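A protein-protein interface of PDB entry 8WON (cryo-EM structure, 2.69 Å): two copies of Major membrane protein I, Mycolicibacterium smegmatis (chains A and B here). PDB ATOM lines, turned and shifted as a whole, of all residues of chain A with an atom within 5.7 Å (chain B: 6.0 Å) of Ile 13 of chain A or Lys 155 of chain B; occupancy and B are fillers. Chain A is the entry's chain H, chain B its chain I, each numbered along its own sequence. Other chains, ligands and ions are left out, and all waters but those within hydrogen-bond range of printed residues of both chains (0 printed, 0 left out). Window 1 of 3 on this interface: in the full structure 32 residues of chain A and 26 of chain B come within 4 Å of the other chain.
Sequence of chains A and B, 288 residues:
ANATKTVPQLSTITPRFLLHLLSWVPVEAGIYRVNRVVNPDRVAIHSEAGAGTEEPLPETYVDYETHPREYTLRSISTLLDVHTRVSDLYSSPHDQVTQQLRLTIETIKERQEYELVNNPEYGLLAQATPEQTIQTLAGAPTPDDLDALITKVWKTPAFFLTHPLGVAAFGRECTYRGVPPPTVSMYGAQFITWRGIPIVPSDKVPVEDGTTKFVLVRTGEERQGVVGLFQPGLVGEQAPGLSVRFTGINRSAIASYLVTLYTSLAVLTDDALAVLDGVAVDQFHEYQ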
ATOM      1  N   LEU A  10     -36.226 -27.136 -11.784  1.00  0.00           N
ATOM      2  CA  LEU A  10     -35.423 -27.649 -12.886  1.00  0.00           C
ATOM      3  C   LEU A  10     -33.953 -27.567 -12.498  1.00  0.00           C
ATOM      4  O   LEU A  10     -33.460 -26.489 -12.155  1.00  0.00           O
ATOM      5  CB  LEU A  10     -35.696 -26.855 -14.160  1.00  0.00           C
ATOM      6  CG  LEU A  10     -35.302 -27.439 -15.514  1.00  0.00           C
ATOM      7  CD1 LEU A  10     -35.803 -28.857 -15.660  1.00  0.00           C
ATOM      8  CD2 LEU A  10     -35.851 -26.565 -16.617  1.00  0.00           C
ATOM      9  N   SER A  11     -33.257 -28.701 -12.547  1.00  0.00           N
ATOM     10  CA  SER A  11     -31.864 -28.735 -12.123  1.00  0.00           C
ATOM     11  C   SER A  11     -30.911 -28.170 -13.166  1.00  0.00           C
ATOM     12  O   SER A  11     -29.759 -27.874 -12.832  1.00  0.00           O
ATOM     13  CB  SER A  11     -31.445 -30.161 -11.777  1.00  0.00           C
ATOM     14  OG  SER A  11     -31.324 -30.962 -12.937  1.00  0.00           O
ATOM     15  N   THR A  12     -31.356 -28.005 -14.406  1.00  0.00           N
ATOM     16  CA  THR A  12     -30.503 -27.501 -15.471  1.00  0.00           C
ATOM     17  C   THR A  12     -30.554 -25.987 -15.613  1.00  0.00           C
ATOM     18  O   THR A  12     -29.944 -25.452 -16.539  1.00  0.00           O
ATOM     19  CB  THR A  12     -30.873 -28.152 -16.803  1.00  0.00           C
ATOM     20  OG1 THR A  12     -32.217 -27.808 -17.149  1.00  0.00           O
ATOM     21  CG2 THR A  12     -30.756 -29.648 -16.708  1.00  0.00           C
ATOM     22  N   ILE A  13     -31.261 -25.287 -14.730  1.00  0.00           N
ATOM     23  CA  ILE A  13     -31.266 -23.830 -14.770  1.00  0.00           C
ATOM     24  C   ILE A  13     -29.933 -23.322 -14.240  1.00  0.00           C
ATOM     25  O   ILE A  13     -29.581 -23.550 -13.079  1.00  0.00           O
ATOM     26  CB  ILE A  13     -32.438 -23.258 -13.962  1.00  0.00           C
ATOM     27  CG1 ILE A  13     -33.773 -23.682 -14.569  1.00  0.00           C
ATOM     28  CG2 ILE A  13     -32.352 -21.749 -13.893  1.00  0.00           C
ATOM     29  CD1 ILE A  13     -34.965 -23.089 -13.867  1.00  0.00           C
ATOM     30  N   THR A  14     -29.186 -22.635 -15.088  1.00  0.00           N
ATOM     31  CA  THR A  14     -27.918 -22.033 -14.726  1.00  0.00           C
ATOM     32  C   THR A  14     -28.059 -20.521 -14.668  1.00  0.00           C
ATOM     33  O   THR A  14     -28.992 -19.953 -15.243  1.00  0.00           O
ATOM     34  CB  THR A  14     -26.817 -22.412 -15.726  1.00  0.00           C
ATOM     35  OG1 THR A  14     -27.126 -21.871 -17.012  1.00  0.00           O
ATOM     36  CG2 THR A  14     -26.681 -23.915 -15.830  1.00  0.00           C
ATOM     37  N   PRO A  15     -27.168 -19.834 -13.950  1.00  0.00           N
ATOM     38  CA  PRO A  15     -27.275 -18.368 -13.859  1.00  0.00           C
ATOM     39  C   PRO A  15     -27.186 -17.655 -15.197  1.00  0.00           C
ATOM     40  O   PRO A  15     -27.709 -16.542 -15.311  1.00  0.00           O
ATOM     41  CB  PRO A  15     -26.113 -17.984 -12.938  1.00  0.00           C
ATOM     42  CG  PRO A  15     -25.292 -19.198 -12.769  1.00  0.00           C
ATOM     43  CD  PRO A  15     -26.144 -20.369 -13.043  1.00  0.00           C
ATOM     44  N   ARG A  16     -26.541 -18.250 -16.201  1.00  0.00           N
ATOM     45  CA  ARG A  16     -26.450 -17.694 -17.553  1.00  0.00           C
ATOM     46  C   ARG A  16     -25.865 -16.283 -17.529  1.00  0.00           C
ATOM     47  O   ARG A  16     -26.476 -15.317 -17.981  1.00  0.00           O
ATOM     48  CB  ARG A  16     -27.810 -17.714 -18.255  1.00  0.00           C
ATOM     49  CG  ARG A  16     -28.279 -19.099 -18.631  1.00  0.00           C
ATOM     50  CD  ARG A  16     -29.607 -19.067 -19.347  1.00  0.00           C
ATOM     51  NE  ARG A  16     -30.602 -18.261 -18.652  1.00  0.00           N
ATOM     52  CZ  ARG A  16     -31.725 -18.739 -18.134  1.00  0.00           C
ATOM     53  NH1 ARG A  16     -32.017 -20.026 -18.187  1.00  0.00           N
ATOM     54  NH2 ARG A  16     -32.575 -17.902 -17.550  1.00  0.00           N
ATOM     55  N   ARG A 102     -43.131 -21.468 -18.545  1.00  0.00           N
ATOM     56  CA  ARG A 102     -41.952 -20.956 -17.853  1.00  0.00           C
ATOM     57  C   ARG A 102     -40.759 -21.895 -18.012  1.00  0.00           C
ATOM     58  O   ARG A 102     -39.634 -21.458 -18.293  1.00  0.00           O
ATOM     59  CB  ARG A 102     -42.269 -20.742 -16.378  1.00  0.00           C
ATOM     60  CG  ARG A 102     -41.184 -20.026 -15.620  1.00  0.00           C
ATOM     61  CD  ARG A 102     -41.515 -19.923 -14.157  1.00  0.00           C
ATOM     62  NE  ARG A 102     -41.811 -21.225 -13.575  1.00  0.00           N
ATOM     63  CZ  ARG A 102     -40.914 -22.000 -12.983  1.00  0.00           C
ATOM     64  NH1 ARG A 102     -39.649 -21.635 -12.878  1.00  0.00           N
ATOM     65  NH2 ARG A 102     -41.298 -23.169 -12.485  1.00  0.00           N
ATOM     66  N   LEU A 103     -40.987 -23.196 -17.832  1.00  0.00           N
ATOM     67  CA  LEU A 103     -39.902 -24.159 -17.968  1.00  0.00           C
ATOM     68  C   LEU A 103     -39.398 -24.224 -19.405  1.00  0.00           C
ATOM     69  O   LEU A 103     -38.187 -24.344 -19.640  1.00  0.00           O
ATOM     70  CB  LEU A 103     -40.362 -25.535 -17.494  1.00  0.00           C
ATOM     71  CG  LEU A 103     -40.847 -25.623 -16.045  1.00  0.00           C
ATOM     72  CD1 LEU A 103     -41.586 -26.926 -15.817  1.00  0.00           C
ATOM     73  CD2 LEU A 103     -39.703 -25.467 -15.064  1.00  0.00           C
ATOM     74  N   GLU A 106     -37.145 -21.225 -19.950  1.00  0.00           N
ATOM     75  CA  GLU A 106     -35.835 -21.412 -19.327  1.00  0.00           C
ATOM     76  C   GLU A 106     -34.956 -22.346 -20.150  1.00  0.00           C
ATOM     77  O   GLU A 106     -33.760 -22.085 -20.337  1.00  0.00           O
ATOM     78  CB  GLU A 106     -35.988 -21.945 -17.907  1.00  0.00           C
ATOM     79  CG  GLU A 106     -36.786 -21.057 -16.996  1.00  0.00           C
ATOM     80  CD  GLU A 106     -35.926 -20.039 -16.296  1.00  0.00           C
ATOM     81  OE1 GLU A 106     -34.693 -20.211 -16.294  1.00  0.00           O
ATOM     82  OE2 GLU A 106     -36.482 -19.069 -15.745  1.00  0.00           O
ATOM     83  N   GLU A 110     -31.310 -21.511 -21.955  1.00  0.00           N
ATOM     84  CA  GLU A 110     -30.111 -22.330 -21.773  1.00  0.00           C
ATOM     85  C   GLU A 110     -29.547 -22.775 -23.116  1.00  0.00           C
ATOM     86  O   GLU A 110     -28.325 -22.768 -23.324  1.00  0.00           O
ATOM     87  CB  GLU A 110     -30.420 -23.546 -20.906  1.00  0.00           C
ATOM     88  CG  GLU A 110     -30.982 -23.235 -19.532  1.00  0.00           C
ATOM     89  CD  GLU A 110     -30.007 -22.521 -18.630  1.00  0.00           C
ATOM     90  OE1 GLU A 110     -28.787 -22.730 -18.778  1.00  0.00           O
ATOM     91  OE2 GLU A 110     -30.463 -21.748 -17.768  1.00  0.00           O
ATOM     92  N   ILE B 150     -16.361 -25.503  -4.257  1.00  0.00           N
ATOM     93  CA  ILE B 150     -16.989 -24.449  -5.051  1.00  0.00           C
ATOM     94  C   ILE B 150     -17.384 -24.976  -6.424  1.00  0.00           C
ATOM     95  O   ILE B 150     -18.422 -24.594  -6.968  1.00  0.00           O
ATOM     96  CB  ILE B 150     -16.068 -23.221  -5.153  1.00  0.00           C
ATOM     97  CG1 ILE B 150     -15.865 -22.600  -3.775  1.00  0.00           C
ATOM     98  CG2 ILE B 150     -16.671 -22.191  -6.077  1.00  0.00           C
ATOM     99  CD1 ILE B 150     -14.843 -21.496  -3.747  1.00  0.00           C
ATOM    100  N   LYS B 152     -18.523 -27.844  -6.992  1.00  0.00           N
ATOM    101  CA  LYS B 152     -19.773 -28.590  -6.842  1.00  0.00           C
ATOM    102  C   LYS B 152     -20.989 -27.679  -6.660  1.00  0.00           C
ATOM    103  O   LYS B 152     -22.107 -28.077  -7.002  1.00  0.00           O
ATOM    104  CB  LYS B 152     -19.665 -29.569  -5.680  1.00  0.00           C
ATOM    105  CG  LYS B 152     -18.513 -30.526  -5.813  1.00  0.00           C
ATOM    106  CD  LYS B 152     -18.981 -31.912  -6.161  1.00  0.00           C
ATOM    107  CE  LYS B 152     -17.989 -32.590  -7.082  1.00  0.00           C
ATOM    108  NZ  LYS B 152     -18.318 -34.023  -7.295  1.00  0.00           N
ATOM    109  N   VAL B 153     -20.813 -26.476  -6.115  1.00  0.00           N
ATOM    110  CA  VAL B 153     -21.916 -25.541  -5.892  1.00  0.00           C
ATOM    111  C   VAL B 153     -21.652 -24.228  -6.620  1.00  0.00           C
ATOM    112  O   VAL B 153     -21.936 -23.149  -6.094  1.00  0.00           O
ATOM    113  CB  VAL B 153     -22.185 -25.304  -4.387  1.00  0.00           C
ATOM    114  CG1 VAL B 153     -23.574 -24.730  -4.161  1.00  0.00           C
ATOM    115  CG2 VAL B 153     -22.080 -26.590  -3.620  1.00  0.00           C
ATOM    116  N   TRP B 154     -21.077 -24.300  -7.822  1.00  0.00           N
ATOM    117  CA  TRP B 154     -20.624 -23.100  -8.522  1.00  0.00           C
ATOM    118  C   TRP B 154     -21.737 -22.094  -8.807  1.00  0.00           C
ATOM    119  O   TRP B 154     -21.437 -20.914  -9.017  1.00  0.00           O
ATOM    120  CB  TRP B 154     -19.924 -23.487  -9.825  1.00  0.00           C
ATOM    121  CG  TRP B 154     -20.813 -24.051 -10.888  1.00  0.00           C
ATOM    122  CD1 TRP B 154     -21.151 -25.357 -11.065  1.00  0.00           C
ATOM    123  CD2 TRP B 154     -21.460 -23.326 -11.939  1.00  0.00           C
ATOM    124  NE1 TRP B 154     -21.972 -25.491 -12.150  1.00  0.00           N
ATOM    125  CE2 TRP B 154     -22.179 -24.257 -12.705  1.00  0.00           C
ATOM    126  CE3 TRP B 154     -21.504 -21.976 -12.301  1.00  0.00           C
ATOM    127  CZ2 TRP B 154     -22.934 -23.886 -13.811  1.00  0.00           C
ATOM    128  CZ3 TRP B 154     -22.252 -21.610 -13.394  1.00  0.00           C
ATOM    129  CH2 TRP B 154     -22.955 -22.560 -14.138  1.00  0.00           C
ATOM    130  N   LYS B 155     -23.001 -22.505  -8.827  1.00  0.00           N
ATOM    131  CA  LYS B 155     -24.092 -21.552  -9.031  1.00  0.00           C
ATOM    132  C   LYS B 155     -24.391 -20.867  -7.704  1.00  0.00           C
ATOM    133  O   LYS B 155     -25.151 -21.367  -6.879  1.00  0.00           O
ATOM    134  CB  LYS B 155     -25.339 -22.234  -9.574  1.00  0.00           C
ATOM    135  CG  LYS B 155     -25.131 -23.150 -10.744  1.00  0.00           C
ATOM    136  CD  LYS B 155     -26.450 -23.759 -11.152  1.00  0.00           C
ATOM    137  CE  LYS B 155     -26.250 -25.022 -11.954  1.00  0.00           C
ATOM    138  NZ  LYS B 155     -27.526 -25.508 -12.529  1.00  0.00           N
ATOM    139  N   THR B 156     -23.763 -19.711  -7.496  1.00  0.00           N
ATOM    140  CA  THR B 156     -23.999 -18.785  -6.392  1.00  0.00           C
ATOM    141  C   THR B 156     -23.944 -19.514  -5.049  1.00  0.00           C
ATOM    142  O   THR B 156     -24.983 -19.825  -4.457  1.00  0.00           O
ATOM    143  CB  THR B 156     -25.335 -18.062  -6.603  1.00  0.00           C
ATOM    144  OG1 THR B 156     -25.182 -17.113  -7.662  1.00  0.00           O
ATOM    145  CG2 THR B 156     -25.728 -17.248  -5.372  1.00  0.00           C
ATOM    146  N   PRO B 157     -22.758 -19.880  -4.566  1.00  0.00           N
ATOM    147  CA  PRO B 157     -22.653 -20.338  -3.177  1.00  0.00           C
ATOM    148  C   PRO B 157     -22.803 -19.166  -2.219  1.00  0.00           C
ATOM    149  O   PRO B 157     -22.339 -18.059  -2.489  1.00  0.00           O
ATOM    150  CB  PRO B 157     -21.252 -20.953  -3.100  1.00  0.00           C
ATOM    151  CG  PRO B 157     -20.679 -20.873  -4.473  1.00  0.00           C
ATOM    152  CD  PRO B 157     -21.455 -19.882  -5.247  1.00  0.00           C
ATOM    153  N   ARG B 218     -26.114 -22.981  -0.957  1.00  0.00           N
ATOM    154  CA  ARG B 218     -26.828 -21.886  -1.599  1.00  0.00           C
ATOM    155  C   ARG B 218     -28.235 -21.818  -1.027  1.00  0.00           C
ATOM    156  O   ARG B 218     -28.961 -22.816  -1.044  1.00  0.00           O
ATOM    157  CB  ARG B 218     -26.892 -22.075  -3.113  1.00  0.00           C
ATOM    158  CG  ARG B 218     -27.811 -21.097  -3.817  1.00  0.00           C
ATOM    159  CD  ARG B 218     -27.842 -21.338  -5.307  1.00  0.00           C
ATOM    160  NE  ARG B 218     -28.739 -22.425  -5.676  1.00  0.00           N
ATOM    161  CZ  ARG B 218     -28.390 -23.485  -6.387  1.00  0.00           C
ATOM    162  NH1 ARG B 218     -27.148 -23.663  -6.800  1.00  0.00           N
ATOM    163  NH2 ARG B 218     -29.311 -24.392  -6.693  1.00  0.00           N
ATOM    164  N   GLN B 224     -33.717 -21.753  -6.325  1.00  0.00           N
ATOM    165  CA  GLN B 224     -33.689 -23.206  -6.165  1.00  0.00           C
ATOM    166  C   GLN B 224     -32.595 -23.644  -5.192  1.00  0.00           C
ATOM    167  O   GLN B 224     -31.799 -24.538  -5.480  1.00  0.00           O
ATOM    168  CB  GLN B 224     -33.529 -23.905  -7.517  1.00  0.00           C
ATOM    169  CG  GLN B 224     -34.315 -23.273  -8.652  1.00  0.00           C
ATOM    170  CD  GLN B 224     -34.230 -24.066  -9.934  1.00  0.00           C
ATOM    171  OE1 GLN B 224     -35.242 -24.513 -10.467  1.00  0.00           O
ATOM    172  NE2 GLN B 224     -33.017 -24.243 -10.442  1.00  0.00           N
ATOM    173  N   ASP B 271     -27.877 -29.754  -6.337  1.00  0.00           N
ATOM    174  CA  ASP B 271     -26.627 -29.025  -6.495  1.00  0.00           C
ATOM    175  C   ASP B 271     -26.586 -27.733  -5.695  1.00  0.00           C
ATOM    176  O   ASP B 271     -25.740 -26.878  -5.964  1.00  0.00           O
ATOM    177  CB  ASP B 271     -26.367 -28.736  -7.977  1.00  0.00           C
ATOM    178  CG  ASP B 271     -27.556 -28.094  -8.668  1.00  0.00           C
ATOM    179  OD1 ASP B 271     -28.555 -28.801  -8.921  1.00  0.00           O
ATOM    180  OD2 ASP B 271     -27.496 -26.882  -8.965  1.00  0.00           O
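The side-chain hydroxyl (OG1) of Thr 14 of chain A lies within hydrogen-bond range of the side-chain carboxylate (OE1) of Glu 110 of chain A, 2.6 Å away.
O of Lys 155 of chain B lies within hydrogen-bond range of NH1 of Arg 218 of chain B, at 3.0 Å.
NZ of Lys 155 of chain B lies within salt-bridge range of OD2 of Asp 271 of chain B, at 3.8 Å.
The guanidinium group (NH2) of Arg 218 of chain B sits at hydrogen-bond distance from the backbone carbonyl oxygen (O) of Gln 224 of chain B (2.8 Å).
The backbone carbonyl oxygen (O) of Leu 10 of chain A sits at hydrogen-bond distance from the side-chain amide nitrogen (NE2) of Gln 224 of chain B, at 2.9 Å.
O of Ser 11 of chain A sits at hydrogen-bond distance from NZ of Lys 155 of chain B (3.3 Å).
NZ of Lys 155 of chain B is in hydrogen-bond range of O of Ile 13 of chain A.
Ile 13 of chain A touches Gln 224 of chain B.
CG2 of Thr 14 of chain A touches NZ of Lys 155 of chain B, 3.8 Å away.
Pro 15 of chain A touches Trp 154 of chain B (CG to CZ3, 3.9 Å).
Pro 15 of chain A touches Lys 155 of chain B (CD to CG, 3.7 Å).
Of the printed residues of chain B, Leu 10 of chain A touches Gln 224.
Of chain B, only Lys 155 (2.9 Å) and Gln 224 (3.7 Å) come within 4 Å of Ile 13 of chain A.
Of the printed residues of chain B, Thr 14 of chain A touches Lys 155.
Of the printed residues of chain B, Pro 15 of chain A touches Trp 154 and Lys 155.
Lys 155 of chain B touches four residues of chain A.
Printed residues of chain A within 4 Å of Gln 224 of chain B: Leu 10 and Ile 13.
The nearest residue of chain B that does not touch Ile 13 of chain A is Asp 271 of chain B (5.7 Å).
The nearest printed residue of chain B that does not touch Ser 11 of chain A is Asp 271 of chain B (4.2 Å).
No position is printed for both chains.
Of the 7 pairs that touch across the chains among the printed residues, none has its exchanged pair printed and touching as well.
Hydrophobic or aromatic side chains of chain A within 4 Å of the printed part of chain B: Ile 13 and Pro 15.
Of the 10 printed residues of chain B, 3 touch a printed residue of chain A.
Hydrophobic or aromatic side chains of chain B that line the printed part of chain A: Trp 154.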
